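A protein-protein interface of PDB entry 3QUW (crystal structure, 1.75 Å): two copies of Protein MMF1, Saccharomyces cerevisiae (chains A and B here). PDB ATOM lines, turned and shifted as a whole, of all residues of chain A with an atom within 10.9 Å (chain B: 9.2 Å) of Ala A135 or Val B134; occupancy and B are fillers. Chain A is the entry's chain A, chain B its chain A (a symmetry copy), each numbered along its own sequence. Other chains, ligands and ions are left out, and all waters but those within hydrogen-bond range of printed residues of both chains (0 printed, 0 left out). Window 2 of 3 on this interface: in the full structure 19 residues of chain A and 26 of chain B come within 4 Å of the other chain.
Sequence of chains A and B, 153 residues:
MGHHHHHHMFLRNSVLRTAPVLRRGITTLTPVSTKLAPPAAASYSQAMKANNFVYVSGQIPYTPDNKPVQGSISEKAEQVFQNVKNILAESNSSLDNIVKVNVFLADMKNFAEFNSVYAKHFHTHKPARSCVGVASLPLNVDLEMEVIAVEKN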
ATOM      1  N   VAL A 103      22.000   9.061 -35.555  1.00  0.00           N
ATOM      2  CA  VAL A 103      23.459   8.970 -35.641  1.00  0.00           C
ATOM      3  C   VAL A 103      24.030   9.618 -34.391  1.00  0.00           C
ATOM      4  O   VAL A 103      23.639  10.719 -34.044  1.00  0.00           O
ATOM      5  CB  VAL A 103      23.982   9.709 -36.897  1.00  0.00           C
ATOM      6  CG1 VAL A 103      25.524   9.667 -36.966  1.00  0.00           C
ATOM      7  CG2 VAL A 103      23.352   9.110 -38.176  1.00  0.00           C
ATOM      8  N   PHE A 104      24.928   8.912 -33.712  1.00  0.00           N
ATOM      9  CA  PHE A 104      25.630   9.468 -32.564  1.00  0.00           C
ATOM     10  C   PHE A 104      27.108   9.499 -32.907  1.00  0.00           C
ATOM     11  O   PHE A 104      27.683   8.473 -33.271  1.00  0.00           O
ATOM     12  CB  PHE A 104      25.370   8.631 -31.298  1.00  0.00           C
ATOM     13  CG  PHE A 104      23.910   8.513 -30.947  1.00  0.00           C
ATOM     14  CD1 PHE A 104      23.164   7.447 -31.418  1.00  0.00           C
ATOM     15  CD2 PHE A 104      23.295   9.483 -30.173  1.00  0.00           C
ATOM     16  CE1 PHE A 104      21.799   7.318 -31.108  1.00  0.00           C
ATOM     17  CE2 PHE A 104      21.918   9.378 -29.851  1.00  0.00           C
ATOM     18  CZ  PHE A 104      21.182   8.290 -30.324  1.00  0.00           C
ATOM     19  N   LEU A 105      27.713  10.683 -32.830  1.00  0.00           N
ATOM     20  CA  LEU A 105      29.122  10.843 -33.124  1.00  0.00           C
ATOM     21  C   LEU A 105      29.902  11.303 -31.887  1.00  0.00           C
ATOM     22  O   LEU A 105      29.478  12.215 -31.177  1.00  0.00           O
ATOM     23  CB  LEU A 105      29.311  11.854 -34.278  1.00  0.00           C
ATOM     24  CG  LEU A 105      29.034  11.389 -35.710  1.00  0.00           C
ATOM     25  CD1 LEU A 105      28.937  12.588 -36.614  1.00  0.00           C
ATOM     26  CD2 LEU A 105      30.180  10.514 -36.183  1.00  0.00           C
ATOM     27  N   ALA A 106      31.038  10.664 -31.629  1.00  0.00           N
ATOM     28  CA  ALA A 106      31.889  11.055 -30.504  1.00  0.00           C
ATOM     29  C   ALA A 106      32.507  12.448 -30.730  1.00  0.00           C
ATOM     30  O   ALA A 106      32.893  13.140 -29.771  1.00  0.00           O
ATOM     31  CB  ALA A 106      32.966  10.001 -30.273  1.00  0.00           C
ATOM     32  N   ASP A 107      32.595  12.858 -31.994  1.00  0.00           N
ATOM     33  CA  ASP A 107      33.126  14.175 -32.344  1.00  0.00           C
ATOM     34  C   ASP A 107      32.418  14.681 -33.586  1.00  0.00           C
ATOM     35  O   ASP A 107      32.515  14.080 -34.662  1.00  0.00           O
ATOM     36  CB  ASP A 107      34.636  14.080 -32.585  1.00  0.00           C
ATOM     37  CG  ASP A 107      35.266  15.405 -32.981  1.00  0.00           C
ATOM     38  OD1 ASP A 107      36.288  15.348 -33.701  1.00  0.00           O
ATOM     39  OD2 ASP A 107      34.763  16.487 -32.601  1.00  0.00           O
ATOM     40  N   MET A 108      31.712  15.794 -33.431  1.00  0.00           N
ATOM     41  CA  MET A 108      30.908  16.349 -34.519  1.00  0.00           C
ATOM     42  C   MET A 108      31.751  16.926 -35.642  1.00  0.00           C
ATOM     43  O   MET A 108      31.235  17.219 -36.714  1.00  0.00           O
ATOM     44  CB  MET A 108      29.910  17.382 -33.998  1.00  0.00           C
ATOM     45  CG  MET A 108      28.596  16.772 -33.538  1.00  0.00           C
ATOM     46  SD  MET A 108      27.629  15.942 -34.824  1.00  0.00           S
ATOM     47  CE  MET A 108      27.205  17.286 -35.897  1.00  0.00           C
ATOM     48  N   ASN A 110      33.718  15.138 -37.143  1.00  0.00           N
ATOM     49  CA  ASN A 110      33.706  14.032 -38.090  1.00  0.00           C
ATOM     50  C   ASN A 110      32.430  13.947 -38.909  1.00  0.00           C
ATOM     51  O   ASN A 110      32.282  13.064 -39.753  1.00  0.00           O
ATOM     52  CB  ASN A 110      33.938  12.713 -37.359  1.00  0.00           C
ATOM     53  CG  ASN A 110      35.318  12.624 -36.765  1.00  0.00           C
ATOM     54  OD1 ASN A 110      35.486  12.212 -35.614  1.00  0.00           O
ATOM     55  ND2 ASN A 110      36.324  13.027 -37.539  1.00  0.00           N
ATOM     56  N   VAL A 132      23.574  13.673 -33.383  1.00  0.00           N
ATOM     57  CA  VAL A 132      24.033  14.398 -32.185  1.00  0.00           C
ATOM     58  C   VAL A 132      25.464  14.018 -31.817  1.00  0.00           C
ATOM     59  O   VAL A 132      25.902  12.904 -32.091  1.00  0.00           O
ATOM     60  CB  VAL A 132      23.099  14.223 -30.946  1.00  0.00           C
ATOM     61  CG1 VAL A 132      21.717  14.810 -31.208  1.00  0.00           C
ATOM     62  CG2 VAL A 132      22.949  12.774 -30.592  1.00  0.00           C
ATOM     63  N   GLY A 133      26.178  14.964 -31.222  1.00  0.00           N
ATOM     64  CA  GLY A 133      27.536  14.721 -30.697  1.00  0.00           C
ATOM     65  C   GLY A 133      27.495  14.333 -29.233  1.00  0.00           C
ATOM     66  O   GLY A 133      27.002  15.095 -28.400  1.00  0.00           O
ATOM     67  N   VAL A 134      28.002  13.141 -28.920  1.00  0.00           N
ATOM     68  CA  VAL A 134      27.947  12.592 -27.574  1.00  0.00           C
ATOM     69  C   VAL A 134      29.301  12.719 -26.887  1.00  0.00           C
ATOM     70  O   VAL A 134      30.298  13.047 -27.532  1.00  0.00           O
ATOM     71  CB  VAL A 134      27.444  11.110 -27.574  1.00  0.00           C
ATOM     72  CG1 VAL A 134      25.964  11.039 -27.993  1.00  0.00           C
ATOM     73  CG2 VAL A 134      28.269  10.236 -28.491  1.00  0.00           C
ATOM     74  N   ALA A 135      29.321  12.487 -25.582  1.00  0.00           N
ATOM     75  CA  ALA A 135      30.557  12.544 -24.812  1.00  0.00           C
ATOM     76  C   ALA A 135      31.422  11.298 -25.062  1.00  0.00           C
ATOM     77  O   ALA A 135      32.642  11.386 -25.187  1.00  0.00           O
ATOM     78  CB  ALA A 135      30.242  12.702 -23.334  1.00  0.00           C
ATOM     79  N   SER A 136      30.781  10.143 -25.165  1.00  0.00           N
ATOM     80  CA  SER A 136      31.484   8.873 -25.301  1.00  0.00           C
ATOM     81  C   SER A 136      30.540   7.809 -25.831  1.00  0.00           C
ATOM     82  O   SER A 136      29.318   7.952 -25.760  1.00  0.00           O
ATOM     83  CB  SER A 136      32.051   8.435 -23.946  1.00  0.00           C
ATOM     84  OG  SER A 136      31.036   8.449 -22.951  1.00  0.00           O
ATOM     85  N   LEU A 137      31.114   6.757 -26.396  1.00  0.00           N
ATOM     86  CA  LEU A 137      30.324   5.668 -26.961  1.00  0.00           C
ATOM     87  C   LEU A 137      30.882   4.357 -26.440  1.00  0.00           C
ATOM     88  O   LEU A 137      32.012   4.339 -25.961  1.00  0.00           O
ATOM     89  CB  LEU A 137      30.366   5.726 -28.484  1.00  0.00           C
ATOM     90  CG  LEU A 137      29.548   6.851 -29.120  1.00  0.00           C
ATOM     91  CD1 LEU A 137      29.817   6.889 -30.605  1.00  0.00           C
ATOM     92  CD2 LEU A 137      28.062   6.659 -28.822  1.00  0.00           C
ATOM     93  N   PRO A 138      30.093   3.270 -26.492  1.00  0.00           N
ATOM     94  CA  PRO A 138      30.565   1.952 -26.039  1.00  0.00           C
ATOM     95  C   PRO A 138      31.886   1.560 -26.682  1.00  0.00           C
ATOM     96  O   PRO A 138      32.090   1.778 -27.877  1.00  0.00           O
ATOM     97  CB  PRO A 138      29.463   1.020 -26.527  1.00  0.00           C
ATOM     98  CG  PRO A 138      28.230   1.873 -26.465  1.00  0.00           C
ATOM     99  CD  PRO A 138      28.715   3.180 -27.020  1.00  0.00           C
ATOM    100  N   LEU A 139      32.780   0.996 -25.876  1.00  0.00           N
ATOM    101  CA  LEU A 139      34.092   0.548 -26.343  1.00  0.00           C
ATOM    102  C   LEU A 139      34.931   1.674 -26.969  1.00  0.00           C
ATOM    103  O   LEU A 139      35.833   1.416 -27.769  1.00  0.00           O
ATOM    104  CB  LEU A 139      33.962  -0.673 -27.283  1.00  0.00           C
ATOM    105  CG  LEU A 139      33.051  -1.851 -26.879  1.00  0.00           C
ATOM    106  CD1 LEU A 139      33.093  -2.948 -27.930  1.00  0.00           C
ATOM    107  CD2 LEU A 139      33.372  -2.435 -25.477  1.00  0.00           C
ATOM    108  N   ASN A 140      34.634   2.918 -26.572  1.00  0.00           N
ATOM    109  CA  ASN A 140      35.331   4.108 -27.044  1.00  0.00           C
ATOM    110  C   ASN A 140      35.337   4.283 -28.575  1.00  0.00           C
ATOM    111  O   ASN A 140      36.263   4.864 -29.142  1.00  0.00           O
ATOM    112  CB  ASN A 140      36.754   4.136 -26.455  1.00  0.00           C
ATOM    113  CG  ASN A 140      37.319   5.528 -26.350  1.00  0.00           C
ATOM    114  OD1 ASN A 140      36.621   6.481 -25.962  1.00  0.00           O
ATOM    115  ND2 ASN A 140      38.604   5.663 -26.687  1.00  0.00           N
ATOM    116  N   VAL A 141      34.291   3.801 -29.251  1.00  0.00           N
ATOM    117  CA  VAL A 141      34.197   3.969 -30.715  1.00  0.00           C
ATOM    118  C   VAL A 141      33.865   5.410 -31.113  1.00  0.00           C
ATOM    119  O   VAL A 141      33.528   6.246 -30.253  1.00  0.00           O
ATOM    120  CB  VAL A 141      33.190   2.999 -31.362  1.00  0.00           C
ATOM    121  CG1 VAL A 141      33.603   1.552 -31.121  1.00  0.00           C
ATOM    122  CG2 VAL A 141      31.791   3.258 -30.845  1.00  0.00           C
ATOM    123  N   ASP A 142      33.960   5.692 -32.417  1.00  0.00           N
ATOM    124  CA  ASP A 142      33.788   7.046 -32.936  1.00  0.00           C
ATOM    125  C   ASP A 142      32.353   7.343 -33.375  1.00  0.00           C
ATOM    126  O   ASP A 142      31.963   8.512 -33.504  1.00  0.00           O
ATOM    127  CB  ASP A 142      34.726   7.278 -34.121  1.00  0.00           C
ATOM    128  CG  ASP A 142      36.183   7.451 -33.691  1.00  0.00           C
ATOM    129  OD1 ASP A 142      36.433   8.164 -32.700  1.00  0.00           O
ATOM    130  OD2 ASP A 142      37.075   6.872 -34.348  1.00  0.00           O
ATOM    131  N   LEU A 143      31.582   6.287 -33.637  1.00  0.00           N
ATOM    132  CA  LEU A 143      30.210   6.466 -34.095  1.00  0.00           C
ATOM    133  C   LEU A 143      29.341   5.278 -33.744  1.00  0.00           C
ATOM    134  O   LEU A 143      29.816   4.145 -33.617  1.00  0.00           O
ATOM    135  CB  LEU A 143      30.156   6.766 -35.604  1.00  0.00           C
ATOM    136  CG  LEU A 143      30.579   5.743 -36.644  1.00  0.00           C
ATOM    137  CD1 LEU A 143      29.652   5.772 -37.882  1.00  0.00           C
ATOM    138  CD2 LEU A 143      32.039   5.957 -37.050  1.00  0.00           C
ATOM    139  N   GLU A 144      28.063   5.562 -33.555  1.00  0.00           N
ATOM    140  CA  GLU A 144      27.055   4.548 -33.312  1.00  0.00           C
ATOM    141  C   GLU A 144      25.834   4.980 -34.115  1.00  0.00           C
ATOM    142  O   GLU A 144      25.485   6.157 -34.125  1.00  0.00           O
ATOM    143  CB  GLU A 144      26.718   4.445 -31.828  1.00  0.00           C
ATOM    144  CG  GLU A 144      25.703   3.358 -31.482  1.00  0.00           C
ATOM    145  CD  GLU A 144      25.428   3.262 -29.979  1.00  0.00           C
ATOM    146  OE1 GLU A 144      26.217   3.809 -29.161  1.00  0.00           O
ATOM    147  OE2 GLU A 144      24.406   2.656 -29.598  1.00  0.00           O
ATOM    148  N   VAL B 103      19.662   3.773 -23.397  1.00  0.00           N
ATOM    149  CA  VAL B 103      20.323   4.070 -22.124  1.00  0.00           C
ATOM    150  C   VAL B 103      21.226   5.271 -22.350  1.00  0.00           C
ATOM    151  O   VAL B 103      21.990   5.287 -23.300  1.00  0.00           O
ATOM    152  CB  VAL B 103      21.168   2.864 -21.649  1.00  0.00           C
ATOM    153  CG1 VAL B 103      21.913   3.189 -20.336  1.00  0.00           C
ATOM    154  CG2 VAL B 103      20.275   1.612 -21.486  1.00  0.00           C
ATOM    155  N   PHE B 104      21.107   6.277 -21.489  1.00  0.00           N
ATOM    156  CA  PHE B 104      21.993   7.430 -21.531  1.00  0.00           C
ATOM    157  C   PHE B 104      22.756   7.465 -20.219  1.00  0.00           C
ATOM    158  O   PHE B 104      22.151   7.463 -19.148  1.00  0.00           O
ATOM    159  CB  PHE B 104      21.199   8.731 -21.746  1.00  0.00           C
ATOM    160  CG  PHE B 104      20.371   8.726 -23.005  1.00  0.00           C
ATOM    161  CD1 PHE B 104      19.052   8.303 -22.969  1.00  0.00           C
ATOM    162  CD2 PHE B 104      20.925   9.117 -24.211  1.00  0.00           C
ATOM    163  CE1 PHE B 104      18.262   8.286 -24.132  1.00  0.00           C
ATOM    164  CE2 PHE B 104      20.150   9.103 -25.398  1.00  0.00           C
ATOM    165  CZ  PHE B 104      18.818   8.686 -25.344  1.00  0.00           C
ATOM    166  N   LEU B 105      24.086   7.455 -20.304  1.00  0.00           N
ATOM    167  CA  LEU B 105      24.927   7.494 -19.124  1.00  0.00           C
ATOM    168  C   LEU B 105      25.774   8.772 -19.085  1.00  0.00           C
ATOM    169  O   LEU B 105      26.376   9.160 -20.087  1.00  0.00           O
ATOM    170  CB  LEU B 105      25.840   6.248 -19.085  1.00  0.00           C
ATOM    171  CG  LEU B 105      25.236   4.912 -18.647  1.00  0.00           C
ATOM    172  CD1 LEU B 105      26.176   3.795 -19.009  1.00  0.00           C
ATOM    173  CD2 LEU B 105      25.045   4.918 -17.140  1.00  0.00           C
ATOM    174  N   ALA B 106      25.815   9.422 -17.928  1.00  0.00           N
ATOM    175  CA  ALA B 106      26.635  10.624 -17.762  1.00  0.00           C
ATOM    176  C   ALA B 106      28.136  10.288 -17.838  1.00  0.00           C
ATOM    177  O   ALA B 106      28.970  11.159 -18.147  1.00  0.00           O
ATOM    178  CB  ALA B 106      26.286  11.316 -16.449  1.00  0.00           C
ATOM    179  N   ASP B 107      28.477   9.032 -17.565  1.00  0.00           N
ATOM    180  CA  ASP B 107      29.864   8.572 -17.638  1.00  0.00           C
ATOM    181  C   ASP B 107      29.882   7.120 -18.072  1.00  0.00           C
ATOM    182  O   ASP B 107      29.367   6.241 -17.372  1.00  0.00           O
ATOM    183  CB  ASP B 107      30.539   8.736 -16.274  1.00  0.00           C
ATOM    184  CG  ASP B 107      31.981   8.256 -16.255  1.00  0.00           C
ATOM    185  OD1 ASP B 107      32.420   7.837 -15.160  1.00  0.00           O
ATOM    186  OD2 ASP B 107      32.672   8.280 -17.298  1.00  0.00           O
ATOM    187  N   MET B 108      30.487   6.874 -19.228  1.00  0.00           N
ATOM    188  CA  MET B 108      30.506   5.534 -19.812  1.00  0.00           C
ATOM    189  C   MET B 108      31.381   4.563 -19.038  1.00  0.00           C
ATOM    190  O   MET B 108      31.322   3.361 -19.266  1.00  0.00           O
ATOM    191  CB  MET B 108      30.911   5.578 -21.285  1.00  0.00           C
ATOM    192  CG  MET B 108      29.738   5.808 -22.225  1.00  0.00           C
ATOM    193  SD  MET B 108      28.475   4.511 -22.228  1.00  0.00           S
ATOM    194  CE  MET B 108      29.367   3.125 -22.878  1.00  0.00           C
ATOM    195  N   LYS B 109      32.172   5.090 -18.111  1.00  0.00           N
ATOM    196  CA  LYS B 109      32.932   4.255 -17.186  1.00  0.00           C
ATOM    197  C   LYS B 109      31.997   3.469 -16.289  1.00  0.00           C
ATOM    198  O   LYS B 109      32.374   2.415 -15.779  1.00  0.00           O
ATOM    199  CB  LYS B 109      33.869   5.094 -16.319  1.00  0.00           C
ATOM    200  CG  LYS B 109      35.134   5.519 -17.025  1.00  0.00           C
ATOM    201  CD  LYS B 109      36.208   5.922 -16.023  1.00  0.00           C
ATOM    202  CE  LYS B 109      36.045   7.359 -15.519  1.00  0.00           C
ATOM    203  NZ  LYS B 109      37.175   7.774 -14.604  1.00  0.00           N
ATOM    204  N   CYS B 131      23.138   2.473 -26.317  1.00  0.00           N
ATOM    205  CA  CYS B 131      23.701   3.053 -25.099  1.00  0.00           C
ATOM    206  C   CYS B 131      24.670   4.130 -25.520  1.00  0.00           C
ATOM    207  O   CYS B 131      25.527   3.886 -26.365  1.00  0.00           O
ATOM    208  CB  CYS B 131      24.454   1.988 -24.307  1.00  0.00           C
ATOM    209  SG  CYS B 131      23.453   0.586 -23.819  1.00  0.00           S
ATOM    210  N   VAL B 132      24.527   5.320 -24.953  1.00  0.00           N
ATOM    211  CA  VAL B 132      25.436   6.428 -25.290  1.00  0.00           C
ATOM    212  C   VAL B 132      25.854   7.206 -24.047  1.00  0.00           C
ATOM    213  O   VAL B 132      25.107   7.273 -23.075  1.00  0.00           O
ATOM    214  CB  VAL B 132      24.867   7.406 -26.367  1.00  0.00           C
ATOM    215  CG1 VAL B 132      24.656   6.701 -27.701  1.00  0.00           C
ATOM    216  CG2 VAL B 132      23.561   7.989 -25.917  1.00  0.00           C
ATOM    217  N   GLY B 133      27.058   7.761 -24.090  1.00  0.00           N
ATOM    218  CA  GLY B 133      27.564   8.644 -23.020  1.00  0.00           C
ATOM    219  C   GLY B 133      27.275  10.099 -23.329  1.00  0.00           C
ATOM    220  O   GLY B 133      27.716  10.618 -24.354  1.00  0.00           O
ATOM    221  N   VAL B 134      26.522  10.755 -22.446  1.00  0.00           N
ATOM    222  CA  VAL B 134      26.082  12.126 -22.654  1.00  0.00           C
ATOM    223  C   VAL B 134      26.911  13.089 -21.812  1.00  0.00           C
ATOM    224  O   VAL B 134      27.671  12.659 -20.943  1.00  0.00           O
ATOM    225  CB  VAL B 134      24.553  12.292 -22.369  1.00  0.00           C
ATOM    226  CG1 VAL B 134      23.719  11.541 -23.425  1.00  0.00           C
ATOM    227  CG2 VAL B 134      24.179  11.798 -20.990  1.00  0.00           C
ATOM    228  N   ALA B 135      26.780  14.377 -22.093  1.00  0.00           N
ATOM    229  CA  ALA B 135      27.493  15.402 -21.343  1.00  0.00           C
ATOM    230  C   ALA B 135      26.850  15.623 -19.963  1.00  0.00           C
ATOM    231  O   ALA B 135      27.541  15.790 -18.960  1.00  0.00           O
ATOM    232  CB  ALA B 135      27.534  16.696 -22.139  1.00  0.00           C
ATOM    233  N   SER B 136      25.526  15.593 -19.915  1.00  0.00           N
ATOM    234  CA  SER B 136      24.786  15.888 -18.694  1.00  0.00           C
ATOM    235  C   SER B 136      23.367  15.360 -18.804  1.00  0.00           C
ATOM    236  O   SER B 136      22.871  15.097 -19.901  1.00  0.00           O
ATOM    237  CB  SER B 136      24.759  17.400 -18.443  1.00  0.00           C
ATOM    238  OG  SER B 136      24.299  18.089 -19.599  1.00  0.00           O
ATOM    239  N   LEU B 137      22.729  15.171 -17.659  1.00  0.00           N
ATOM    240  CA  LEU B 137      21.366  14.654 -17.620  1.00  0.00           C
ATOM    241  C   LEU B 137      20.546  15.543 -16.705  1.00  0.00           C
ATOM    242  O   LEU B 137      21.127  16.281 -15.914  1.00  0.00           O
ATOM    243  CB  LEU B 137      21.369  13.208 -17.137  1.00  0.00           C
ATOM    244  CG  LEU B 137      21.891  12.181 -18.143  1.00  0.00           C
ATOM    245  CD1 LEU B 137      21.994  10.831 -17.475  1.00  0.00           C
ATOM    246  CD2 LEU B 137      20.983  12.134 -19.371  1.00  0.00           C
ATOM    247  N   PRO B 138      19.207  15.512 -16.827  1.00  0.00           N
ATOM    248  CA  PRO B 138      18.335  16.317 -15.957  1.00  0.00           C
ATOM    249  C   PRO B 138      18.641  16.111 -14.482  1.00  0.00           C
ATOM    250  O   PRO B 138      18.878  14.985 -14.043  1.00  0.00           O
ATOM    251  CB  PRO B 138      16.951  15.764 -16.274  1.00  0.00           C
ATOM    252  CG  PRO B 138      17.059  15.350 -17.712  1.00  0.00           C
ATOM    253  CD  PRO B 138      18.405  14.687 -17.756  1.00  0.00           C
ATOM    254  N   VAL B 141      21.676  13.829 -12.753  1.00  0.00           N
ATOM    255  CA  VAL B 141      21.707  12.383 -12.452  1.00  0.00           C
ATOM    256  C   VAL B 141      22.758  11.642 -13.281  1.00  0.00           C
ATOM    257  O   VAL B 141      23.344  12.210 -14.222  1.00  0.00           O
ATOM    258  CB  VAL B 141      20.331  11.712 -12.622  1.00  0.00           C
ATOM    259  CG1 VAL B 141      19.308  12.326 -11.675  1.00  0.00           C
ATOM    260  CG2 VAL B 141      19.865  11.805 -14.059  1.00  0.00           C
ATOM    261  N   ASP B 142      22.991  10.373 -12.928  1.00  0.00           N
ATOM    262  CA  ASP B 142      24.045   9.572 -13.545  1.00  0.00           C
ATOM    263  C   ASP B 142      23.550   8.742 -14.732  1.00  0.00           C
ATOM    264  O   ASP B 142      24.351   8.293 -15.564  1.00  0.00           O
ATOM    265  CB  ASP B 142      24.667   8.634 -12.511  1.00  0.00           C
ATOM    266  CG  ASP B 142      25.577   9.370 -11.526  1.00  0.00           C
ATOM    267  OD1 ASP B 142      26.362  10.232 -11.966  1.00  0.00           O
ATOM    268  OD2 ASP B 142      25.503   9.081 -10.311  1.00  0.00           O
ATOM    269  N   LEU B 143      22.238   8.510 -14.788  1.00  0.00           N
ATOM    270  CA  LEU B 143      21.674   7.701 -15.861  1.00  0.00           C
ATOM    271  C   LEU B 143      20.225   8.051 -16.127  1.00  0.00           C
ATOM    272  O   LEU B 143      19.500   8.511 -15.240  1.00  0.00           O
ATOM    273  CB  LEU B 143      21.836   6.197 -15.575  1.00  0.00           C
ATOM    274  CG  LEU B 143      21.125   5.515 -14.419  1.00  0.00           C
ATOM    275  CD1 LEU B 143      20.623   4.105 -14.809  1.00  0.00           C
ATOM    276  CD2 LEU B 143      22.033   5.450 -13.188  1.00  0.00           C
ATOM    277  N   GLU B 144      19.828   7.859 -17.373  1.00  0.00           N
ATOM    278  CA  GLU B 144      18.455   8.038 -17.803  1.00  0.00           C
ATOM    279  C   GLU B 144      18.169   6.889 -18.762  1.00  0.00           C
ATOM    280  O   GLU B 144      19.002   6.562 -19.601  1.00  0.00           O
ATOM    281  CB  GLU B 144      18.262   9.382 -18.495  1.00  0.00           C
ATOM    282  CG  GLU B 144      16.826   9.673 -18.928  1.00  0.00           C
ATOM    283  CD  GLU B 144      16.671  11.049 -19.579  1.00  0.00           C
ATOM    284  OE1 GLU B 144      17.579  11.914 -19.442  1.00  0.00           O
ATOM    285  OE2 GLU B 144      15.648  11.277 -20.256  1.00  0.00           O
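Of chain B, only Gly B133 and Val B134 come within 4 Å of Ala A135.
Of chain A, only Ala A135 (3.5 Å) comes within 4 Å of Val B134.
Ser A136 touches three residues of chain B.
Phe B104 touches none of the printed residues of chain A.
No residue of chain A comes within 4 Å of Ala B106.
Of chain A, only Val A134 (3.3 Å), Ala A135 (2.8 Å) and Ser A136 (2.8 Å) come within 4 Å of Gly B133.
No residue of chain A comes within 4 Å of Ala B135.
Ser B136 touches none of the printed residues of chain A.
Of the printed residues of chain B, Glu A144 touches Cys B131 and Val B132.
Printed residues of chain B within 4 Å of Phe A104: Val B132.
Of the printed residues of chain B, Leu A137 touches Val B132.
Printed residues of chain A within 4 Å of Cys B131: Pro A138 (3.3 Å) and Glu A144 (2.9 Å).
Of the printed residues of chain A, Met B108 touches Ser A136 (3.0 Å) and Pro A138 (3.6 Å).
Leu B137 touches none of the printed residues of chain A.
Val B141 touches none of the printed residues of chain A.
The nearest residue of chain B that does not touch Ala A135 is Ala B135 (4.04 Å).
The nearest printed residue of chain A that does not touch Cys B131 is Leu A137 (4.5 Å).
The backbone NH (N) of Val B134 lies within hydrogen-bond range of the backbone carbonyl oxygen (O) of Leu B105, 2.9 Å away.
The backbone NH (N) of Leu B105 sits at hydrogen-bond distance from the backbone carbonyl oxygen (O) of Val B132, 3.0 Å away.
The backbone carbonyl oxygen (O) of Glu A144 is in hydrogen-bond range of the backbone NH (N) of Phe A104, at 2.8 Å.
The backbone carbonyl oxygen (O) of Leu A105 sits at hydrogen-bond distance from the backbone NH (N) of Val A134, 2.9 Å away.
The backbone carbonyl oxygen (O) of Val B103 lies within hydrogen-bond range of the backbone NH (N) of Val B132 (3.0 Å).
Phe A104 touches Val B132, but with the chains exchanged Val A132 does not touch Phe B104 (6.9 Å).
Ala A135 touches Gly B133, but with the chains exchanged Gly A133 does not touch Ala B135 (6.4 Å).
Leu A137 touches Val B132, but with the chains exchanged Val A132 does not touch Leu B137 (11.4 Å).
Glu A144 touches Val B132, but with the chains exchanged Val A132 does not touch Glu B144 (12.4 Å).
Of the 12 pairs that touch across the chains among the printed residues, none has its exchanged pair printed and touching as well.
N of Ala A135 lies within hydrogen-bond range of O of Gly B133 (2.8 Å).
O of Ser A136 sits at hydrogen-bond distance from N of Gly B133 (2.8 Å).
The backbone carbonyl oxygen of Cys B131 lies close to the side-chain carboxylate of Glu A144 (2.9 Å).
Of the 19 printed residues of chain B, 5 touch a printed residue of chain A.
Hydrophobic or aromatic side chains of chain B within 4 Å of the printed part of chain A: Met B108 and Val B132.
Among the printed residues, 12 pairs touch across the chains.
Among the printed residues, pairs that only touch across the chains: Phe A104 with Val B132 (3.8 Å), Val A134 with Gly B133 (3.3 Å), Ala A135 with Val B134 (3.5 Å), Ser A136 with Met B108 (3.0 Å), Ser A136 with Val B132 (3.9 Å), Leu A137 with Val B132 (3.6 Å), Pro A138 with Met B108 (3.6 Å), Pro A138 with Cys B131 (3.3 Å) and Glu A144 with Val B132 (3.6 Å).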
